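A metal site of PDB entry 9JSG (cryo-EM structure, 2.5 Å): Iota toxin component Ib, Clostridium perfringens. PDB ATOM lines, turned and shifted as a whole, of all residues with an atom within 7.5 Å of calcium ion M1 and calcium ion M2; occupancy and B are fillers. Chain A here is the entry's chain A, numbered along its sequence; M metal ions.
The side-chain carboxylate (OE1) of Glu 30 sits close to the side-chain hydroxyl (OG) of Ser 58.
N of Ser 59 sits at hydrogen-bond distance from OG1 of Thr 65 (3.3 Å).
The side-chain hydroxyl (OG) of Ser 59 lies close to the backbone NH (N) of Leu 61 (3.4 Å).
OD2 of Asp 19 is in hydrogen-bond range of N of Asn 24, 2.9 Å away.
The backbone NH of Asp 72 sits at hydrogen-bond distance from the backbone carbonyl oxygen of Ser 63.
The side-chain carboxylate of Asp 72 is in hydrogen-bond range of the side-chain hydroxyl of Thr 65 (3.2 Å).
OD2 of Asp 27 sits close to N of Thr 20 (3.5 Å).
N of Asp 27 lies within hydrogen-bond range of O of Leu 18, at 2.8 Å.
Merely in contact with calcium ion M1: Tyr 60 (3.8 Å) and Pro 26 (3.9 Å).
Of the 26 residues printed, 8 come within 4 Å of calcium ion M1.
The nearest printed residue that does not touch calcium ion M1 is Thr 20 (4.2 Å).
Calcium ion M1 is bound by the side-chain carboxylate of Asp 21, the side-chain carboxylate of Glu 30, the backbone carbonyl oxygen of Ile 25, the side-chain carboxylate of Asp 19, the side-chain carboxylate of Asp 23 and the side-chain carboxylate of Asp 27.
Calcium ion M1 has six donor atoms within binding distance.
Six residues have an atom within 4 Å of calcium ion M2: Asp 21, Asp 23, Glu 30, Ser 59, Glu 62 and Asp 72.
O of Glu 62 binds calcium ion M2 (2.5 Å).
O of Ser 59 binds calcium ion M2 (2.5 Å).
OE1 of Glu 30 binds calcium ion M2 (2.5 Å).
OD2 of Asp 21 is bound to calcium ion M2 (2.6 Å).
OD2 of Asp 72 binds calcium ion M2, 2.6 Å away.
The side-chain carboxylate (OD2) of Asp 23 is bound to calcium ion M2 (2.7 Å).
OE2 of Glu 30 is bound to calcium ion M2 (2.9 Å).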
ATOM      1  N   LEU A  18     -24.867   3.310  -9.435  1.00  0.00           N
ATOM      2  CA  LEU A  18     -23.709   3.915 -10.063  1.00  0.00           C
ATOM      3  C   LEU A  18     -23.862   3.910 -11.573  1.00  0.00           C
ATOM      4  O   LEU A  18     -24.226   2.883 -12.167  1.00  0.00           O
ATOM      5  CB  LEU A  18     -22.440   3.158  -9.655  1.00  0.00           C
ATOM      6  CG  LEU A  18     -21.113   3.878  -9.909  1.00  0.00           C
ATOM      7  CD1 LEU A  18     -21.003   5.139  -9.068  1.00  0.00           C
ATOM      8  CD2 LEU A  18     -19.943   2.944  -9.661  1.00  0.00           C
ATOM      9  N   ASP A  19     -23.600   5.053 -12.199  1.00  0.00           N
ATOM     10  CA  ASP A  19     -23.686   5.231 -13.643  1.00  0.00           C
ATOM     11  C   ASP A  19     -22.391   5.893 -14.109  1.00  0.00           C
ATOM     12  O   ASP A  19     -22.274   7.123 -14.092  1.00  0.00           O
ATOM     13  CB  ASP A  19     -24.916   6.048 -14.031  1.00  0.00           C
ATOM     14  CG  ASP A  19     -25.262   5.908 -15.493  1.00  0.00           C
ATOM     15  OD1 ASP A  19     -24.653   5.060 -16.182  1.00  0.00           O
ATOM     16  OD2 ASP A  19     -26.160   6.645 -15.969  1.00  0.00           O
ATOM     17  N   THR A  20     -21.416   5.072 -14.506  1.00  0.00           N
ATOM     18  CA  THR A  20     -20.101   5.600 -14.859  1.00  0.00           C
ATOM     19  C   THR A  20     -20.142   6.407 -16.151  1.00  0.00           C
ATOM     20  O   THR A  20     -19.577   7.503 -16.226  1.00  0.00           O
ATOM     21  CB  THR A  20     -19.093   4.461 -14.968  1.00  0.00           C
ATOM     22  OG1 THR A  20     -19.232   3.582 -13.843  1.00  0.00           O
ATOM     23  CG2 THR A  20     -17.671   4.998 -15.017  1.00  0.00           C
ATOM     24  N   ASP A  21     -20.805   5.889 -17.178  1.00  0.00           N
ATOM     25  CA  ASP A  21     -20.841   6.539 -18.479  1.00  0.00           C
ATOM     26  C   ASP A  21     -21.994   7.523 -18.628  1.00  0.00           C
ATOM     27  O   ASP A  21     -22.120   8.153 -19.685  1.00  0.00           O
ATOM     28  CB  ASP A  21     -20.926   5.485 -19.595  1.00  0.00           C
ATOM     29  CG  ASP A  21     -21.963   4.418 -19.304  1.00  0.00           C
ATOM     30  OD1 ASP A  21     -22.529   4.433 -18.188  1.00  0.00           O
ATOM     31  OD2 ASP A  21     -22.208   3.564 -20.179  1.00  0.00           O
ATOM     32  N   ASN A  22     -22.812   7.698 -17.582  1.00  0.00           N
ATOM     33  CA  ASN A  22     -23.969   8.598 -17.615  1.00  0.00           C
ATOM     34  C   ASN A  22     -24.875   8.305 -18.816  1.00  0.00           C
ATOM     35  O   ASN A  22     -25.365   9.213 -19.480  1.00  0.00           O
ATOM     36  CB  ASN A  22     -23.537  10.066 -17.609  1.00  0.00           C
ATOM     37  CG  ASN A  22     -22.331  10.321 -16.724  1.00  0.00           C
ATOM     38  OD1 ASN A  22     -21.191  10.090 -17.134  1.00  0.00           O
ATOM     39  ND2 ASN A  22     -22.565  10.760 -15.490  1.00  0.00           N
ATOM     40  N   ASP A  23     -25.099   7.020 -19.073  1.00  0.00           N
ATOM     41  CA  ASP A  23     -25.965   6.574 -20.148  1.00  0.00           C
ATOM     42  C   ASP A  23     -27.364   6.218 -19.645  1.00  0.00           C
ATOM     43  O   ASP A  23     -28.130   5.565 -20.362  1.00  0.00           O
ATOM     44  CB  ASP A  23     -25.342   5.382 -20.882  1.00  0.00           C
ATOM     45  CG  ASP A  23     -25.541   4.078 -20.147  1.00  0.00           C
ATOM     46  OD1 ASP A  23     -25.254   4.022 -18.930  1.00  0.00           O
ATOM     47  OD2 ASP A  23     -25.978   3.095 -20.793  1.00  0.00           O
ATOM     48  N   ASN A  24     -27.703   6.634 -18.422  1.00  0.00           N
ATOM     49  CA  ASN A  24     -29.009   6.489 -17.772  1.00  0.00           C
ATOM     50  C   ASN A  24     -29.312   5.060 -17.352  1.00  0.00           C
ATOM     51  O   ASN A  24     -30.455   4.781 -16.937  1.00  0.00           O
ATOM     52  CB  ASN A  24     -30.151   7.031 -18.635  1.00  0.00           C
ATOM     53  CG  ASN A  24     -30.907   8.158 -17.972  1.00  0.00           C
ATOM     54  OD1 ASN A  24     -30.345   8.906 -17.174  1.00  0.00           O
ATOM     55  ND2 ASN A  24     -32.190   8.290 -18.307  1.00  0.00           N
ATOM     56  N   ILE A  25     -28.361   4.141 -17.443  1.00  0.00           N
ATOM     57  CA  ILE A  25     -28.532   2.765 -17.012  1.00  0.00           C
ATOM     58  C   ILE A  25     -27.425   2.445 -16.007  1.00  0.00           C
ATOM     59  O   ILE A  25     -26.254   2.706 -16.297  1.00  0.00           O
ATOM     60  CB  ILE A  25     -28.499   1.767 -18.179  1.00  0.00           C
ATOM     61  CG1 ILE A  25     -29.372   2.258 -19.331  1.00  0.00           C
ATOM     62  CG2 ILE A  25     -28.949   0.382 -17.719  1.00  0.00           C
ATOM     63  CD1 ILE A  25     -28.938   1.769 -20.700  1.00  0.00           C
ATOM     64  N   PRO A  26     -27.742   1.915 -14.835  1.00  0.00           N
ATOM     65  CA  PRO A  26     -26.699   1.628 -13.840  1.00  0.00           C
ATOM     66  C   PRO A  26     -25.722   0.560 -14.331  1.00  0.00           C
ATOM     67  O   PRO A  26     -26.063  -0.286 -15.167  1.00  0.00           O
ATOM     68  CB  PRO A  26     -27.484   1.143 -12.624  1.00  0.00           C
ATOM     69  CG  PRO A  26     -28.865   1.695 -12.808  1.00  0.00           C
ATOM     70  CD  PRO A  26     -29.099   1.698 -14.287  1.00  0.00           C
ATOM     71  N   ASP A  27     -24.500   0.618 -13.804  1.00  0.00           N
ATOM     72  CA  ASP A  27     -23.457  -0.309 -14.216  1.00  0.00           C
ATOM     73  C   ASP A  27     -23.828  -1.752 -13.884  1.00  0.00           C
ATOM     74  O   ASP A  27     -23.581  -2.664 -14.690  1.00  0.00           O
ATOM     75  CB  ASP A  27     -22.131   0.060 -13.548  1.00  0.00           C
ATOM     76  CG  ASP A  27     -21.715   1.485 -13.834  1.00  0.00           C
ATOM     77  OD1 ASP A  27     -22.423   2.177 -14.598  1.00  0.00           O
ATOM     78  OD2 ASP A  27     -20.692   1.926 -13.275  1.00  0.00           O
ATOM     79  N   ALA A  28     -24.409  -1.988 -12.702  1.00  0.00           N
ATOM     80  CA  ALA A  28     -24.821  -3.337 -12.341  1.00  0.00           C
ATOM     81  C   ALA A  28     -25.916  -3.848 -13.266  1.00  0.00           C
ATOM     82  O   ALA A  28     -25.973  -5.041 -13.572  1.00  0.00           O
ATOM     83  CB  ALA A  28     -25.289  -3.360 -10.879  1.00  0.00           C
ATOM     84  N   TYR A  29     -26.798  -2.945 -13.721  1.00  0.00           N
ATOM     85  CA  TYR A  29     -27.846  -3.349 -14.648  1.00  0.00           C
ATOM     86  C   TYR A  29     -27.281  -3.714 -16.002  1.00  0.00           C
ATOM     87  O   TYR A  29     -27.788  -4.615 -16.681  1.00  0.00           O
ATOM     88  CB  TYR A  29     -28.883  -2.227 -14.784  1.00  0.00           C
ATOM     89  CG  TYR A  29     -29.815  -2.086 -13.597  1.00  0.00           C
ATOM     90  CD1 TYR A  29     -29.593  -2.799 -12.423  1.00  0.00           C
ATOM     91  CD2 TYR A  29     -30.912  -1.229 -13.650  1.00  0.00           C
ATOM     92  CE1 TYR A  29     -30.443  -2.664 -11.337  1.00  0.00           C
ATOM     93  CE2 TYR A  29     -31.761  -1.095 -12.575  1.00  0.00           C
ATOM     94  CZ  TYR A  29     -31.523  -1.808 -11.418  1.00  0.00           C
ATOM     95  N   GLU A  30     -26.218  -3.025 -16.435  1.00  0.00           N
ATOM     96  CA  GLU A  30     -25.611  -3.322 -17.737  1.00  0.00           C
ATOM     97  C   GLU A  30     -24.766  -4.588 -17.694  1.00  0.00           C
ATOM     98  O   GLU A  30     -24.740  -5.352 -18.657  1.00  0.00           O
ATOM     99  CB  GLU A  30     -24.775  -2.137 -18.221  1.00  0.00           C
ATOM    100  CG  GLU A  30     -25.549  -0.839 -18.329  1.00  0.00           C
ATOM    101  CD  GLU A  30     -24.888   0.154 -19.252  1.00  0.00           C
ATOM    102  OE1 GLU A  30     -24.726  -0.164 -20.453  1.00  0.00           O
ATOM    103  OE2 GLU A  30     -24.525   1.257 -18.795  1.00  0.00           O
ATOM    104  N   TYR A  34     -31.075  -6.361 -18.099  1.00  0.00           N
ATOM    105  CA  TYR A  34     -31.984  -5.299 -17.711  1.00  0.00           C
ATOM    106  C   TYR A  34     -33.050  -5.152 -18.780  1.00  0.00           C
ATOM    107  O   TYR A  34     -32.892  -5.621 -19.909  1.00  0.00           O
ATOM    108  CB  TYR A  34     -31.237  -3.972 -17.488  1.00  0.00           C
ATOM    109  CG  TYR A  34     -30.657  -3.359 -18.747  1.00  0.00           C
ATOM    110  CD1 TYR A  34     -29.395  -3.732 -19.204  1.00  0.00           C
ATOM    111  CD2 TYR A  34     -31.361  -2.409 -19.479  1.00  0.00           C
ATOM    112  CE1 TYR A  34     -28.862  -3.175 -20.344  1.00  0.00           C
ATOM    113  CE2 TYR A  34     -30.836  -1.845 -20.619  1.00  0.00           C
ATOM    114  CZ  TYR A  34     -29.582  -2.238 -21.056  1.00  0.00           C
ATOM    115  N   SER A  58     -25.112  -4.508 -22.097  1.00  0.00           N
ATOM    116  CA  SER A  58     -24.302  -3.486 -22.764  1.00  0.00           C
ATOM    117  C   SER A  58     -23.090  -3.182 -21.882  1.00  0.00           C
ATOM    118  O   SER A  58     -22.975  -3.680 -20.754  1.00  0.00           O
ATOM    119  CB  SER A  58     -25.120  -2.222 -23.046  1.00  0.00           C
ATOM    120  OG  SER A  58     -26.086  -2.001 -22.020  1.00  0.00           O
ATOM    121  N   SER A  59     -22.191  -2.362 -22.413  1.00  0.00           N
ATOM    122  CA  SER A  59     -20.976  -1.971 -21.709  1.00  0.00           C
ATOM    123  C   SER A  59     -21.288  -0.823 -20.755  1.00  0.00           C
ATOM    124  O   SER A  59     -21.887   0.180 -21.166  1.00  0.00           O
ATOM    125  CB  SER A  59     -19.881  -1.570 -22.693  1.00  0.00           C
ATOM    126  OG  SER A  59     -18.729  -1.119 -22.010  1.00  0.00           O
ATOM    127  N   TYR A  60     -20.883  -0.966 -19.499  1.00  0.00           N
ATOM    128  CA  TYR A  60     -21.111   0.073 -18.508  1.00  0.00           C
ATOM    129  C   TYR A  60     -20.078   1.191 -18.582  1.00  0.00           C
ATOM    130  O   TYR A  60     -20.211   2.191 -17.860  1.00  0.00           O
ATOM    131  CB  TYR A  60     -21.132  -0.528 -17.097  1.00  0.00           C
ATOM    132  CG  TYR A  60     -19.786  -0.949 -16.562  1.00  0.00           C
ATOM    133  CD1 TYR A  60     -19.245  -2.188 -16.868  1.00  0.00           C
ATOM    134  CD2 TYR A  60     -19.045  -0.110 -15.731  1.00  0.00           C
ATOM    135  CE1 TYR A  60     -18.015  -2.579 -16.379  1.00  0.00           C
ATOM    136  CE2 TYR A  60     -17.816  -0.487 -15.243  1.00  0.00           C
ATOM    137  CZ  TYR A  60     -17.302  -1.728 -15.562  1.00  0.00           C
ATOM    138  N   LEU A  61     -19.050   1.056 -19.415  1.00  0.00           N
ATOM    139  CA  LEU A  61     -18.056   2.093 -19.618  1.00  0.00           C
ATOM    140  C   LEU A  61     -18.234   2.838 -20.941  1.00  0.00           C
ATOM    141  O   LEU A  61     -17.513   3.804 -21.180  1.00  0.00           O
ATOM    142  CB  LEU A  61     -16.645   1.503 -19.569  1.00  0.00           C
ATOM    143  CG  LEU A  61     -16.074   1.209 -18.172  1.00  0.00           C
ATOM    144  CD1 LEU A  61     -14.688   0.594 -18.275  1.00  0.00           C
ATOM    145  CD2 LEU A  61     -16.042   2.476 -17.330  1.00  0.00           C
ATOM    146  N   GLU A  62     -19.176   2.414 -21.784  1.00  0.00           N
ATOM    147  CA  GLU A  62     -19.426   3.047 -23.077  1.00  0.00           C
ATOM    148  C   GLU A  62     -20.885   3.435 -23.158  1.00  0.00           C
ATOM    149  O   GLU A  62     -21.764   2.592 -22.936  1.00  0.00           O
ATOM    150  CB  GLU A  62     -19.047   2.105 -24.229  1.00  0.00           C
ATOM    151  CG  GLU A  62     -18.324   2.786 -25.376  1.00  0.00           C
ATOM    152  CD  GLU A  62     -17.038   3.463 -24.936  1.00  0.00           C
ATOM    153  OE1 GLU A  62     -16.193   2.784 -24.319  1.00  0.00           O
ATOM    154  OE2 GLU A  62     -16.880   4.665 -25.215  1.00  0.00           O
ATOM    155  N   SER A  63     -21.151   4.698 -23.479  1.00  0.00           N
ATOM    156  CA  SER A  63     -22.532   5.152 -23.646  1.00  0.00           C
ATOM    157  C   SER A  63     -23.129   4.636 -24.948  1.00  0.00           C
ATOM    158  O   SER A  63     -24.345   4.390 -25.028  1.00  0.00           O
ATOM    159  CB  SER A  63     -22.605   6.673 -23.580  1.00  0.00           C
ATOM    160  OG  SER A  63     -22.131   7.260 -24.778  1.00  0.00           O
ATOM    161  N   ASN A  64     -22.312   4.476 -25.985  1.00  0.00           N
ATOM    162  CA  ASN A  64     -22.726   3.950 -27.276  1.00  0.00           C
ATOM    163  C   ASN A  64     -21.904   2.690 -27.538  1.00  0.00           C
ATOM    164  O   ASN A  64     -20.811   2.746 -28.095  1.00  0.00           O
ATOM    165  CB  ASN A  64     -22.541   4.978 -28.396  1.00  0.00           C
ATOM    166  CG  ASN A  64     -23.281   6.284 -28.118  1.00  0.00           C
ATOM    167  OD1 ASN A  64     -23.121   6.880 -27.062  1.00  0.00           O
ATOM    168  ND2 ASN A  64     -24.096   6.711 -29.077  1.00  0.00           N
ATOM    169  N   THR A  65     -22.443   1.542 -27.105  1.00  0.00           N
ATOM    170  CA  THR A  65     -21.701   0.284 -27.225  1.00  0.00           C
ATOM    171  C   THR A  65     -21.466  -0.094 -28.685  1.00  0.00           C
ATOM    172  O   THR A  65     -20.369  -0.520 -29.046  1.00  0.00           O
ATOM    173  CB  THR A  65     -22.452  -0.825 -26.495  1.00  0.00           C
ATOM    174  OG1 THR A  65     -22.614  -0.472 -25.116  1.00  0.00           O
ATOM    175  CG2 THR A  65     -21.683  -2.137 -26.589  1.00  0.00           C
ATOM    176  N   THR A  71     -27.490   6.157 -28.119  1.00  0.00           N
ATOM    177  CA  THR A  71     -26.962   5.565 -26.908  1.00  0.00           C
ATOM    178  C   THR A  71     -27.707   4.272 -26.578  1.00  0.00           C
ATOM    179  O   THR A  71     -28.712   3.927 -27.192  1.00  0.00           O
ATOM    180  CB  THR A  71     -27.060   6.541 -25.737  1.00  0.00           C
ATOM    181  OG1 THR A  71     -28.409   6.582 -25.256  1.00  0.00           O
ATOM    182  CG2 THR A  71     -26.640   7.942 -26.172  1.00  0.00           C
ATOM    183  N   ASP A  72     -27.181   3.551 -25.581  1.00  0.00           N
ATOM    184  CA  ASP A  72     -27.768   2.272 -25.194  1.00  0.00           C
ATOM    185  C   ASP A  72     -29.196   2.455 -24.681  1.00  0.00           C
ATOM    186  O   ASP A  72     -30.098   1.684 -25.041  1.00  0.00           O
ATOM    187  CB  ASP A  72     -26.902   1.598 -24.131  1.00  0.00           C
ATOM    188  CG  ASP A  72     -25.525   1.242 -24.657  1.00  0.00           C
ATOM    189  OD1 ASP A  72     -25.391   1.007 -25.876  1.00  0.00           O
ATOM    190  OD2 ASP A  72     -24.582   1.182 -23.840  1.00  0.00           O
ATOM    191  N   TYR A  73     -29.422   3.456 -23.829  1.00  0.00           N
ATOM    192  CA  TYR A  73     -30.761   3.692 -23.300  1.00  0.00           C
ATOM    193  C   TYR A  73     -31.731   4.121 -24.398  1.00  0.00           C
ATOM    194  O   TYR A  73     -32.895   3.711 -24.400  1.00  0.00           O
ATOM    195  CB  TYR A  73     -30.718   4.744 -22.189  1.00  0.00           C
ATOM    196  CG  TYR A  73     -32.082   5.115 -21.653  1.00  0.00           C
ATOM    197  CD1 TYR A  73     -32.737   4.282 -20.760  1.00  0.00           C
ATOM    198  CD2 TYR A  73     -32.714   6.288 -22.049  1.00  0.00           C
ATOM    199  CE1 TYR A  73     -33.988   4.615 -20.269  1.00  0.00           C
ATOM    200  CE2 TYR A  73     -33.959   6.629 -21.557  1.00  0.00           C
ATOM    201  CZ  TYR A  73     -34.591   5.789 -20.672  1.00  0.00           C
ATOM    202  N   PRO A  91     -28.821  -3.060 -27.792  1.00  0.00           N
ATOM    203  CA  PRO A  91     -27.577  -2.271 -27.768  1.00  0.00           C
ATOM    204  C   PRO A  91     -26.429  -2.897 -28.543  1.00  0.00           C
ATOM    205  O   PRO A  91     -25.560  -2.173 -29.030  1.00  0.00           O
ATOM    206  CB  PRO A  91     -27.248  -2.172 -26.265  1.00  0.00           C
ATOM    207  CG  PRO A  91     -28.557  -2.399 -25.579  1.00  0.00           C
ATOM    208  CD  PRO A  91     -29.299  -3.388 -26.431  1.00  0.00           C
HETATM  209 CA    CA M   1     -23.875   2.782 -16.973  1.00  0.00          CA
HETATM  210 CA    CA M   2     -23.681   1.921 -21.480  1.00  0.00          CA
